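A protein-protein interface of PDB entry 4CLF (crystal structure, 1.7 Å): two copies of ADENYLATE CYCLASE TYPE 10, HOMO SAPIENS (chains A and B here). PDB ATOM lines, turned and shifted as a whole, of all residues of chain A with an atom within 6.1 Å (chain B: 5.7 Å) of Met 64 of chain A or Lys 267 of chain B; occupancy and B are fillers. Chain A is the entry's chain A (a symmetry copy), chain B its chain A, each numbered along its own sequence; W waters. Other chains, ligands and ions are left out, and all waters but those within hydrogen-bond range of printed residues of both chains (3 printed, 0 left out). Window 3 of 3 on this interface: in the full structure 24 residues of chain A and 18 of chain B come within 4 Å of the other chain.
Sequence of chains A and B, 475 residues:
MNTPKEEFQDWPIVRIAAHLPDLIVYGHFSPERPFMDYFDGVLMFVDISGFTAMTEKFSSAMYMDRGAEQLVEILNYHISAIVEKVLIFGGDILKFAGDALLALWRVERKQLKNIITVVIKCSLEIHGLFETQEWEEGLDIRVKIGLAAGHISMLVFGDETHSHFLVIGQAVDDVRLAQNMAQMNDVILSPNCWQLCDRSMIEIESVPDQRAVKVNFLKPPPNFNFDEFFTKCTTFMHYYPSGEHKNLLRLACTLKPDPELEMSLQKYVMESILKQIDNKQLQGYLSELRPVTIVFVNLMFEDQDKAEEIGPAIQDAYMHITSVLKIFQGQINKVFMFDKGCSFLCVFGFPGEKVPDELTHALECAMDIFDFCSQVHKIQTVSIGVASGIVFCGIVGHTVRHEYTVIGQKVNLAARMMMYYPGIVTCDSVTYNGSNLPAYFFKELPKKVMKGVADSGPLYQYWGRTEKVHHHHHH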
ATOM      1  N   SER A  60      18.521  20.315 -26.803  1.00  0.00           N
ATOM      2  CA  SER A  60      18.520  21.790 -26.673  1.00  0.00           C
ATOM      3  C   SER A  60      18.153  22.331 -25.268  1.00  0.00           C
ATOM      4  O   SER A  60      17.189  21.855 -24.593  1.00  0.00           O
ATOM      5  CB  SER A  60      17.496  22.340 -27.643  1.00  0.00           C
ATOM      6  OG  SER A  60      17.278  23.703 -27.402  1.00  0.00           O
ATOM      7  N   ALA A  61      18.853  23.382 -24.846  1.00  0.00           N
ATOM      8  CA  ALA A  61      18.482  24.132 -23.669  1.00  0.00           C
ATOM      9  C   ALA A  61      17.063  24.693 -23.697  1.00  0.00           C
ATOM     10  O   ALA A  61      16.551  25.108 -22.653  1.00  0.00           O
ATOM     11  CB  ALA A  61      19.445  25.277 -23.433  1.00  0.00           C
ATOM     12  N   MET A  62      16.444  24.758 -24.871  1.00  0.00           N
ATOM     13  CA  MET A  62      15.049  25.239 -24.955  1.00  0.00           C
ATOM     14  C   MET A  62      14.113  24.370 -24.133  1.00  0.00           C
ATOM     15  O   MET A  62      13.041  24.861 -23.664  1.00  0.00           O
ATOM     16  CB  MET A  62      14.563  25.414 -26.403  1.00  0.00           C
ATOM     17  CG  MET A  62      14.196  24.205 -27.230  1.00  0.00           C
ATOM     18  SD  MET A  62      13.385  24.671 -28.817  1.00  0.00           S
ATOM     19  CE  MET A  62      14.464  25.954 -29.411  1.00  0.00           C
ATOM     20  N   TYR A  63      14.518  23.106 -23.942  1.00  0.00           N
ATOM     21  CA  TYR A  63      13.692  22.108 -23.207  1.00  0.00           C
ATOM     22  C   TYR A  63      13.885  22.119 -21.681  1.00  0.00           C
ATOM     23  O   TYR A  63      13.188  21.401 -20.937  1.00  0.00           O
ATOM     24  CB  TYR A  63      13.807  20.700 -23.764  1.00  0.00           C
ATOM     25  CG  TYR A  63      13.096  20.653 -25.073  1.00  0.00           C
ATOM     26  CD1 TYR A  63      11.726  20.534 -25.115  1.00  0.00           C
ATOM     27  CD2 TYR A  63      13.799  20.857 -26.279  1.00  0.00           C
ATOM     28  CE1 TYR A  63      11.046  20.615 -26.311  1.00  0.00           C
ATOM     29  CE2 TYR A  63      13.161  20.842 -27.500  1.00  0.00           C
ATOM     30  CZ  TYR A  63      11.787  20.736 -27.531  1.00  0.00           C
ATOM     31  OH  TYR A  63      11.119  20.769 -28.723  1.00  0.00           O
ATOM     32  N   MET A  64      14.694  23.059 -21.221  1.00  0.00           N
ATOM     33  CA  MET A  64      14.724  23.419 -19.815  1.00  0.00           C
ATOM     34  C   MET A  64      14.888  22.214 -18.924  1.00  0.00           C
ATOM     35  O   MET A  64      14.227  22.128 -17.895  1.00  0.00           O
ATOM     36  CB  MET A  64      13.461  24.151 -19.412  1.00  0.00           C
ATOM     37  CG  MET A  64      13.467  25.573 -19.916  1.00  0.00           C
ATOM     38  SD  MET A  64      11.851  26.384 -19.866  1.00  0.00           S
ATOM     39  CE  MET A  64      10.810  25.505 -21.048  1.00  0.00           C
ATOM     40  N   ASP A  65      15.813  21.379 -19.233  1.00  0.00           N
ATOM     41  CA  ASP A  65      15.981  20.200 -18.342  1.00  0.00           C
ATOM     42  C   ASP A  65      14.797  19.198 -18.291  1.00  0.00           C
ATOM     43  O   ASP A  65      14.887  18.208 -17.556  1.00  0.00           O
ATOM     44  CB  ASP A  65      16.378  20.571 -16.929  1.00  0.00           C
ATOM     45  CG  ASP A  65      17.601  21.496 -16.906  1.00  0.00           C
ATOM     46  OD1 ASP A  65      18.596  21.200 -17.593  1.00  0.00           O
ATOM     47  OD2 ASP A  65      17.539  22.496 -16.229  1.00  0.00           O
ATOM     48  N   ARG A  66      13.785  19.365 -19.160  1.00  0.00           N
ATOM     49  CA  ARG A  66      12.813  18.293 -19.299  1.00  0.00           C
ATOM     50  C   ARG A  66      12.862  17.710 -20.685  1.00  0.00           C
ATOM     51  O   ARG A  66      11.913  17.172 -21.164  1.00  0.00           O
ATOM     52  CB  ARG A  66      11.368  18.812 -18.959  1.00  0.00           C
ATOM     53  CG  ARG A  66      11.237  19.147 -17.487  1.00  0.00           C
ATOM     54  CD  ARG A  66       9.820  19.508 -17.104  1.00  0.00           C
ATOM     55  NE  ARG A  66       8.867  18.495 -17.357  1.00  0.00           N
ATOM     56  CZ  ARG A  66       8.019  18.406 -18.362  1.00  0.00           C
ATOM     57  NH1 ARG A  66       7.893  19.422 -19.268  1.00  0.00           N
ATOM     58  NH2 ARG A  66       7.237  17.349 -18.486  1.00  0.00           N
ATOM     59  N   GLY A  67      14.044  17.777 -21.350  1.00  0.00           N
ATOM     60  CA  GLY A  67      14.099  17.055 -22.608  1.00  0.00           C
ATOM     61  C   GLY A  67      13.746  15.632 -22.701  1.00  0.00           C
ATOM     62  O   GLY A  67      13.090  15.210 -23.645  1.00  0.00           O
ATOM     63  N   ASP B 159      10.367  35.686 -17.790  1.00  0.00           N
ATOM     64  CA  ASP B 159      11.627  35.615 -18.549  1.00  0.00           C
ATOM     65  C   ASP B 159      11.609  34.401 -19.455  1.00  0.00           C
ATOM     66  O   ASP B 159      10.526  33.882 -19.761  1.00  0.00           O
ATOM     67  CB  ASP B 159      12.801  35.649 -17.572  1.00  0.00           C
ATOM     68  CG  ASP B 159      12.795  34.534 -16.550  1.00  0.00           C
ATOM     69  OD1 ASP B 159      12.172  33.474 -16.777  1.00  0.00           O
ATOM     70  OD2 ASP B 159      13.599  34.594 -15.597  1.00  0.00           O
ATOM     71  N   GLU B 160      12.792  33.896 -19.813  1.00  0.00           N
ATOM     72  CA  GLU B 160      12.873  32.840 -20.763  1.00  0.00           C
ATOM     73  C   GLU B 160      12.453  31.493 -20.164  1.00  0.00           C
ATOM     74  O   GLU B 160      12.146  30.549 -20.918  1.00  0.00           O
ATOM     75  CB  GLU B 160      14.287  32.738 -21.335  1.00  0.00           C
ATOM     76  CG  GLU B 160      14.683  34.076 -22.009  1.00  0.00           C
ATOM     77  CD  GLU B 160      15.563  34.958 -21.092  1.00  0.00           C
ATOM     78  OE1 GLU B 160      15.445  34.903 -19.821  1.00  0.00           O
ATOM     79  OE2 GLU B 160      16.419  35.698 -21.655  1.00  0.00           O
ATOM     80  N   THR B 161      12.470  31.369 -18.847  1.00  0.00           N
ATOM     81  CA  THR B 161      12.161  30.070 -18.195  1.00  0.00           C
ATOM     82  C   THR B 161      10.894  30.082 -17.376  1.00  0.00           C
ATOM     83  O   THR B 161      10.337  29.004 -17.205  1.00  0.00           O
ATOM     84  CB  THR B 161      13.314  29.518 -17.347  1.00  0.00           C
ATOM     85  OG1 THR B 161      13.448  30.259 -16.167  1.00  0.00           O
ATOM     86  CG2 THR B 161      14.606  29.664 -18.037  1.00  0.00           C
ATOM     87  N   HIS B 162      10.396  31.268 -16.942  1.00  0.00           N
ATOM     88  CA  HIS B 162       9.243  31.403 -16.069  1.00  0.00           C
ATOM     89  C   HIS B 162       8.225  32.391 -16.594  1.00  0.00           C
ATOM     90  O   HIS B 162       8.599  33.400 -17.124  1.00  0.00           O
ATOM     91  CB  HIS B 162       9.663  31.781 -14.661  1.00  0.00           C
ATOM     92  CG  HIS B 162      10.534  30.761 -14.010  1.00  0.00           C
ATOM     93  ND1 HIS B 162      11.808  31.040 -13.617  1.00  0.00           N
ATOM     94  CD2 HIS B 162      10.359  29.420 -13.805  1.00  0.00           C
ATOM     95  CE1 HIS B 162      12.367  29.957 -13.128  1.00  0.00           C
ATOM     96  NE2 HIS B 162      11.528  28.943 -13.277  1.00  0.00           N
ATOM     97  N   SER B 163       6.953  32.091 -16.505  1.00  0.00           N
ATOM     98  CA  SER B 163       5.868  32.988 -16.851  1.00  0.00           C
ATOM     99  C   SER B 163       4.837  33.083 -15.726  1.00  0.00           C
ATOM    100  O   SER B 163       4.640  32.140 -14.915  1.00  0.00           O
ATOM    101  CB  SER B 163       5.107  32.494 -18.073  1.00  0.00           C
ATOM    102  OG  SER B 163       6.032  32.365 -19.179  1.00  0.00           O
ATOM    103  N   HIS B 164       4.271  34.261 -15.617  1.00  0.00           N
ATOM    104  CA  HIS B 164       3.185  34.547 -14.701  1.00  0.00           C
ATOM    105  C   HIS B 164       2.125  35.371 -15.420  1.00  0.00           C
ATOM    106  O   HIS B 164       2.433  36.143 -16.342  1.00  0.00           O
ATOM    107  CB  HIS B 164       3.676  35.364 -13.492  1.00  0.00           C
ATOM    108  CG  HIS B 164       4.750  34.703 -12.723  1.00  0.00           C
ATOM    109  ND1 HIS B 164       4.491  33.869 -11.666  1.00  0.00           N
ATOM    110  CD2 HIS B 164       6.083  34.666 -12.910  1.00  0.00           C
ATOM    111  CE1 HIS B 164       5.629  33.327 -11.244  1.00  0.00           C
ATOM    112  NE2 HIS B 164       6.613  33.823 -11.971  1.00  0.00           N
ATOM    113  N   GLU B 262       3.860  22.473 -24.687  1.00  0.00           N
ATOM    114  CA  GLU B 262       4.300  22.123 -23.342  1.00  0.00           C
ATOM    115  C   GLU B 262       5.448  22.980 -22.875  1.00  0.00           C
ATOM    116  O   GLU B 262       5.493  23.319 -21.677  1.00  0.00           O
ATOM    117  CB  GLU B 262       4.692  20.623 -23.326  1.00  0.00           C
ATOM    118  CG  GLU B 262       5.094  20.168 -21.934  1.00  0.00           C
ATOM    119  CD  GLU B 262       5.161  18.633 -21.759  1.00  0.00           C
ATOM    120  OE1 GLU B 262       4.321  17.922 -22.366  1.00  0.00           O
ATOM    121  OE2 GLU B 262       6.075  18.158 -21.023  1.00  0.00           O
ATOM    122  N   MET B 263       6.359  23.299 -23.778  1.00  0.00           N
ATOM    123  CA  MET B 263       7.415  24.250 -23.451  1.00  0.00           C
ATOM    124  C   MET B 263       6.879  25.557 -22.868  1.00  0.00           C
ATOM    125  O   MET B 263       7.435  26.092 -21.922  1.00  0.00           O
ATOM    126  CB  MET B 263       8.396  24.516 -24.624  1.00  0.00           C
ATOM    127  CG  MET B 263       9.571  23.570 -24.590  1.00  0.00           C
ATOM    128  SD  MET B 263      10.769  24.016 -25.903  1.00  0.00           S
ATOM    129  CE  MET B 263      10.305  25.701 -26.136  1.00  0.00           C
ATOM    130  N   SER B 264       5.843  26.082 -23.505  1.00  0.00           N
ATOM    131  CA  SER B 264       5.194  27.313 -23.069  1.00  0.00           C
ATOM    132  C   SER B 264       4.475  27.141 -21.752  1.00  0.00           C
ATOM    133  O   SER B 264       4.648  27.954 -20.811  1.00  0.00           O
ATOM    134  CB  SER B 264       4.174  27.755 -24.131  1.00  0.00           C
ATOM    135  OG  SER B 264       4.900  28.042 -25.284  1.00  0.00           O
ATOM    136  N   LEU B 265       3.683  26.069 -21.629  1.00  0.00           N
ATOM    137  CA  LEU B 265       2.917  25.875 -20.406  1.00  0.00           C
ATOM    138  C   LEU B 265       3.715  25.544 -19.126  1.00  0.00           C
ATOM    139  O   LEU B 265       3.396  26.017 -18.023  1.00  0.00           O
ATOM    140  CB  LEU B 265       1.825  24.781 -20.630  1.00  0.00           C
ATOM    141  CG  LEU B 265       0.805  25.048 -21.718  1.00  0.00           C
ATOM    142  CD1 LEU B 265      -0.158  23.865 -21.731  1.00  0.00           C
ATOM    143  CD2 LEU B 265       0.106  26.384 -21.581  1.00  0.00           C
ATOM    144  N   GLN B 266       4.830  24.849 -19.255  1.00  0.00           N
ATOM    145  CA  GLN B 266       5.544  24.429 -18.091  1.00  0.00           C
ATOM    146  C   GLN B 266       6.163  25.625 -17.420  1.00  0.00           C
ATOM    147  O   GLN B 266       6.447  25.519 -16.239  1.00  0.00           O
ATOM    148  CB  GLN B 266       6.604  23.425 -18.420  1.00  0.00           C
ATOM    149  CG  GLN B 266       7.824  23.988 -19.118  1.00  0.00           C
ATOM    150  CD  GLN B 266       9.033  23.099 -18.944  1.00  0.00           C
ATOM    151  OE1 GLN B 266       9.102  22.037 -19.499  1.00  0.00           O
ATOM    152  NE2 GLN B 266       9.956  23.538 -18.085  1.00  0.00           N
ATOM    153  N   LYS B 267       6.306  26.757 -18.120  1.00  0.00           N
ATOM    154  CA  LYS B 267       6.994  27.949 -17.551  1.00  0.00           C
ATOM    155  C   LYS B 267       6.179  28.571 -16.424  1.00  0.00           C
ATOM    156  O   LYS B 267       6.705  29.288 -15.566  1.00  0.00           O
ATOM    157  CB  LYS B 267       7.254  28.957 -18.633  1.00  0.00           C
ATOM    158  CG  LYS B 267       8.262  28.474 -19.678  1.00  0.00           C
ATOM    159  CD  LYS B 267       8.586  29.603 -20.659  1.00  0.00           C
ATOM    160  CE  LYS B 267       9.477  29.023 -21.766  1.00  0.00           C
ATOM    161  NZ  LYS B 267       9.767  30.051 -22.794  1.00  0.00           N
ATOM    162  N   TYR B 268       4.893  28.192 -16.351  1.00  0.00           N
ATOM    163  CA  TYR B 268       4.003  28.690 -15.316  1.00  0.00           C
ATOM    164  C   TYR B 268       3.999  27.873 -14.037  1.00  0.00           C
ATOM    165  O   TYR B 268       3.436  28.374 -13.029  1.00  0.00           O
ATOM    166  CB  TYR B 268       2.566  28.812 -15.852  1.00  0.00           C
ATOM    167  CG  TYR B 268       2.364  29.780 -16.971  1.00  0.00           C
ATOM    168  CD1 TYR B 268       2.563  29.426 -18.309  1.00  0.00           C
ATOM    169  CD2 TYR B 268       1.917  31.048 -16.714  1.00  0.00           C
ATOM    170  CE1 TYR B 268       2.357  30.293 -19.334  1.00  0.00           C
ATOM    171  CE2 TYR B 268       1.632  31.935 -17.742  1.00  0.00           C
ATOM    172  CZ  TYR B 268       1.880  31.547 -19.063  1.00  0.00           C
ATOM    173  OH  TYR B 268       1.649  32.469 -20.078  1.00  0.00           O
ATOM    174  N   VAL B 269       4.670  26.707 -14.044  1.00  0.00           N
ATOM    175  CA  VAL B 269       4.570  25.724 -13.018  1.00  0.00           C
ATOM    176  C   VAL B 269       5.912  25.558 -12.310  1.00  0.00           C
ATOM    177  O   VAL B 269       6.955  25.476 -12.949  1.00  0.00           O
ATOM    178  CB  VAL B 269       4.075  24.409 -13.640  1.00  0.00           C
ATOM    179  CG1 VAL B 269       3.941  23.371 -12.615  1.00  0.00           C
ATOM    180  CG2 VAL B 269       2.714  24.674 -14.316  1.00  0.00           C
HETATM  181  O   HOH W   1      10.246  26.228 -16.780  1.00  0.00           O
HETATM  182  O   HOH W   2      10.458  21.479 -21.784  1.00  0.00           O
HETATM  183  O   HOH W   3      12.215  22.529 -16.420  1.00  0.00           O
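OE2 of Glu 262 of chain B is in salt-bridge range of NH1 of Arg 66 of chain A, at 2.8 Å. The side-chain sulfur of Met 263 of chain B lies close to the backbone carbonyl oxygen of Met 62 of chain A, at 3.3 Å. The side-chain amide oxygen (OE1) of Gln 266 of chain B lies within hydrogen-bond range of the guanidinium group (NH1) of Arg 66 of chain A (2.9 Å).
The side-chain amino group of Lys 267 of chain B is in hydrogen-bond range of the backbone carbonyl oxygen of Glu 160 of chain B (3.1 Å). OG of Ser 60 of chain A lies within hydrogen-bond range of N of Met 62 of chain A. O of Lys 267 of chain B lies within hydrogen-bond range of N of Ser 163 of chain B, at 3.0 Å.
Among the printed residues, pairs that only touch across the chains: Tyr 63 of chain A with Met 263 of chain B, Met 64 of chain A with Met 263 of chain B, Met 64 of chain A with Gln 266 of chain B and Met 64 of chain A with Lys 267 of chain B.
Of the printed residues of chain B, Tyr 63 of chain A touches Met 263 (3.4 Å). Met 64 of chain A touches three residues of chain B. Printed residues of chain B within 4 Å of Arg 66 of chain A: Glu 262 and Gln 266. Of the printed residues of chain A, Gln 266 of chain B touches Met 64 (3.7 Å) and Arg 66 (2.9 Å). Lys 267 of chain B touches just one residue of chain A: Met 64. Tyr 268 of chain B touches none of the printed residues of chain A. Val 269 of chain B touches none of the printed residues of chain A. The nearest residue of chain B that does not touch Met 64 of chain A is Thr 161 of chain B (4.03 Å). The nearest printed residue of chain A that does not touch Lys 267 of chain B is Met 62 of chain A (5.8 Å).
Printed residues of chain B that touch a printed residue of chain A: Glu 262, Met 263, Gln 266 and Lys 267. Along chain B the printed residues that touch a printed residue of chain A span positions 262 to 267. Of the 8 printed residues of chain A, 4 touch a printed residue of chain B. Hydrophobic or aromatic side chains of chain A within 4 Å of the printed part of chain B: Met 62, Tyr 63 and Met 64. Among the printed residues, Asp or Glu carboxylates within 4 Å of a Lys or Arg side-chain nitrogen of the other chain: Arg 66 of chain A with Glu 262 of chain B (2.8 Å).
No position is printed for both chains.
Water W3 lies within hydrogen-bond range of the backbone carbonyl oxygen (O) of Met 64 of chain A (2.5 Å) and the side-chain amide nitrogen (NE2) of Gln 266 of chain B (3.0 Å). Water W2 lies within hydrogen-bond range of the side-chain amide oxygen of Gln 266 of chain B (2.7 Å) and the backbone carbonyl oxygen of Tyr 63 of chain A (2.9 Å). Water W1 lies within hydrogen-bond range of the backbone carbonyl oxygen (O) of Thr 161 of chain B, the side-chain amide nitrogen (NE2) of Gln 266 of chain B and the side-chain sulfur (SD) of Met 64 of chain A.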
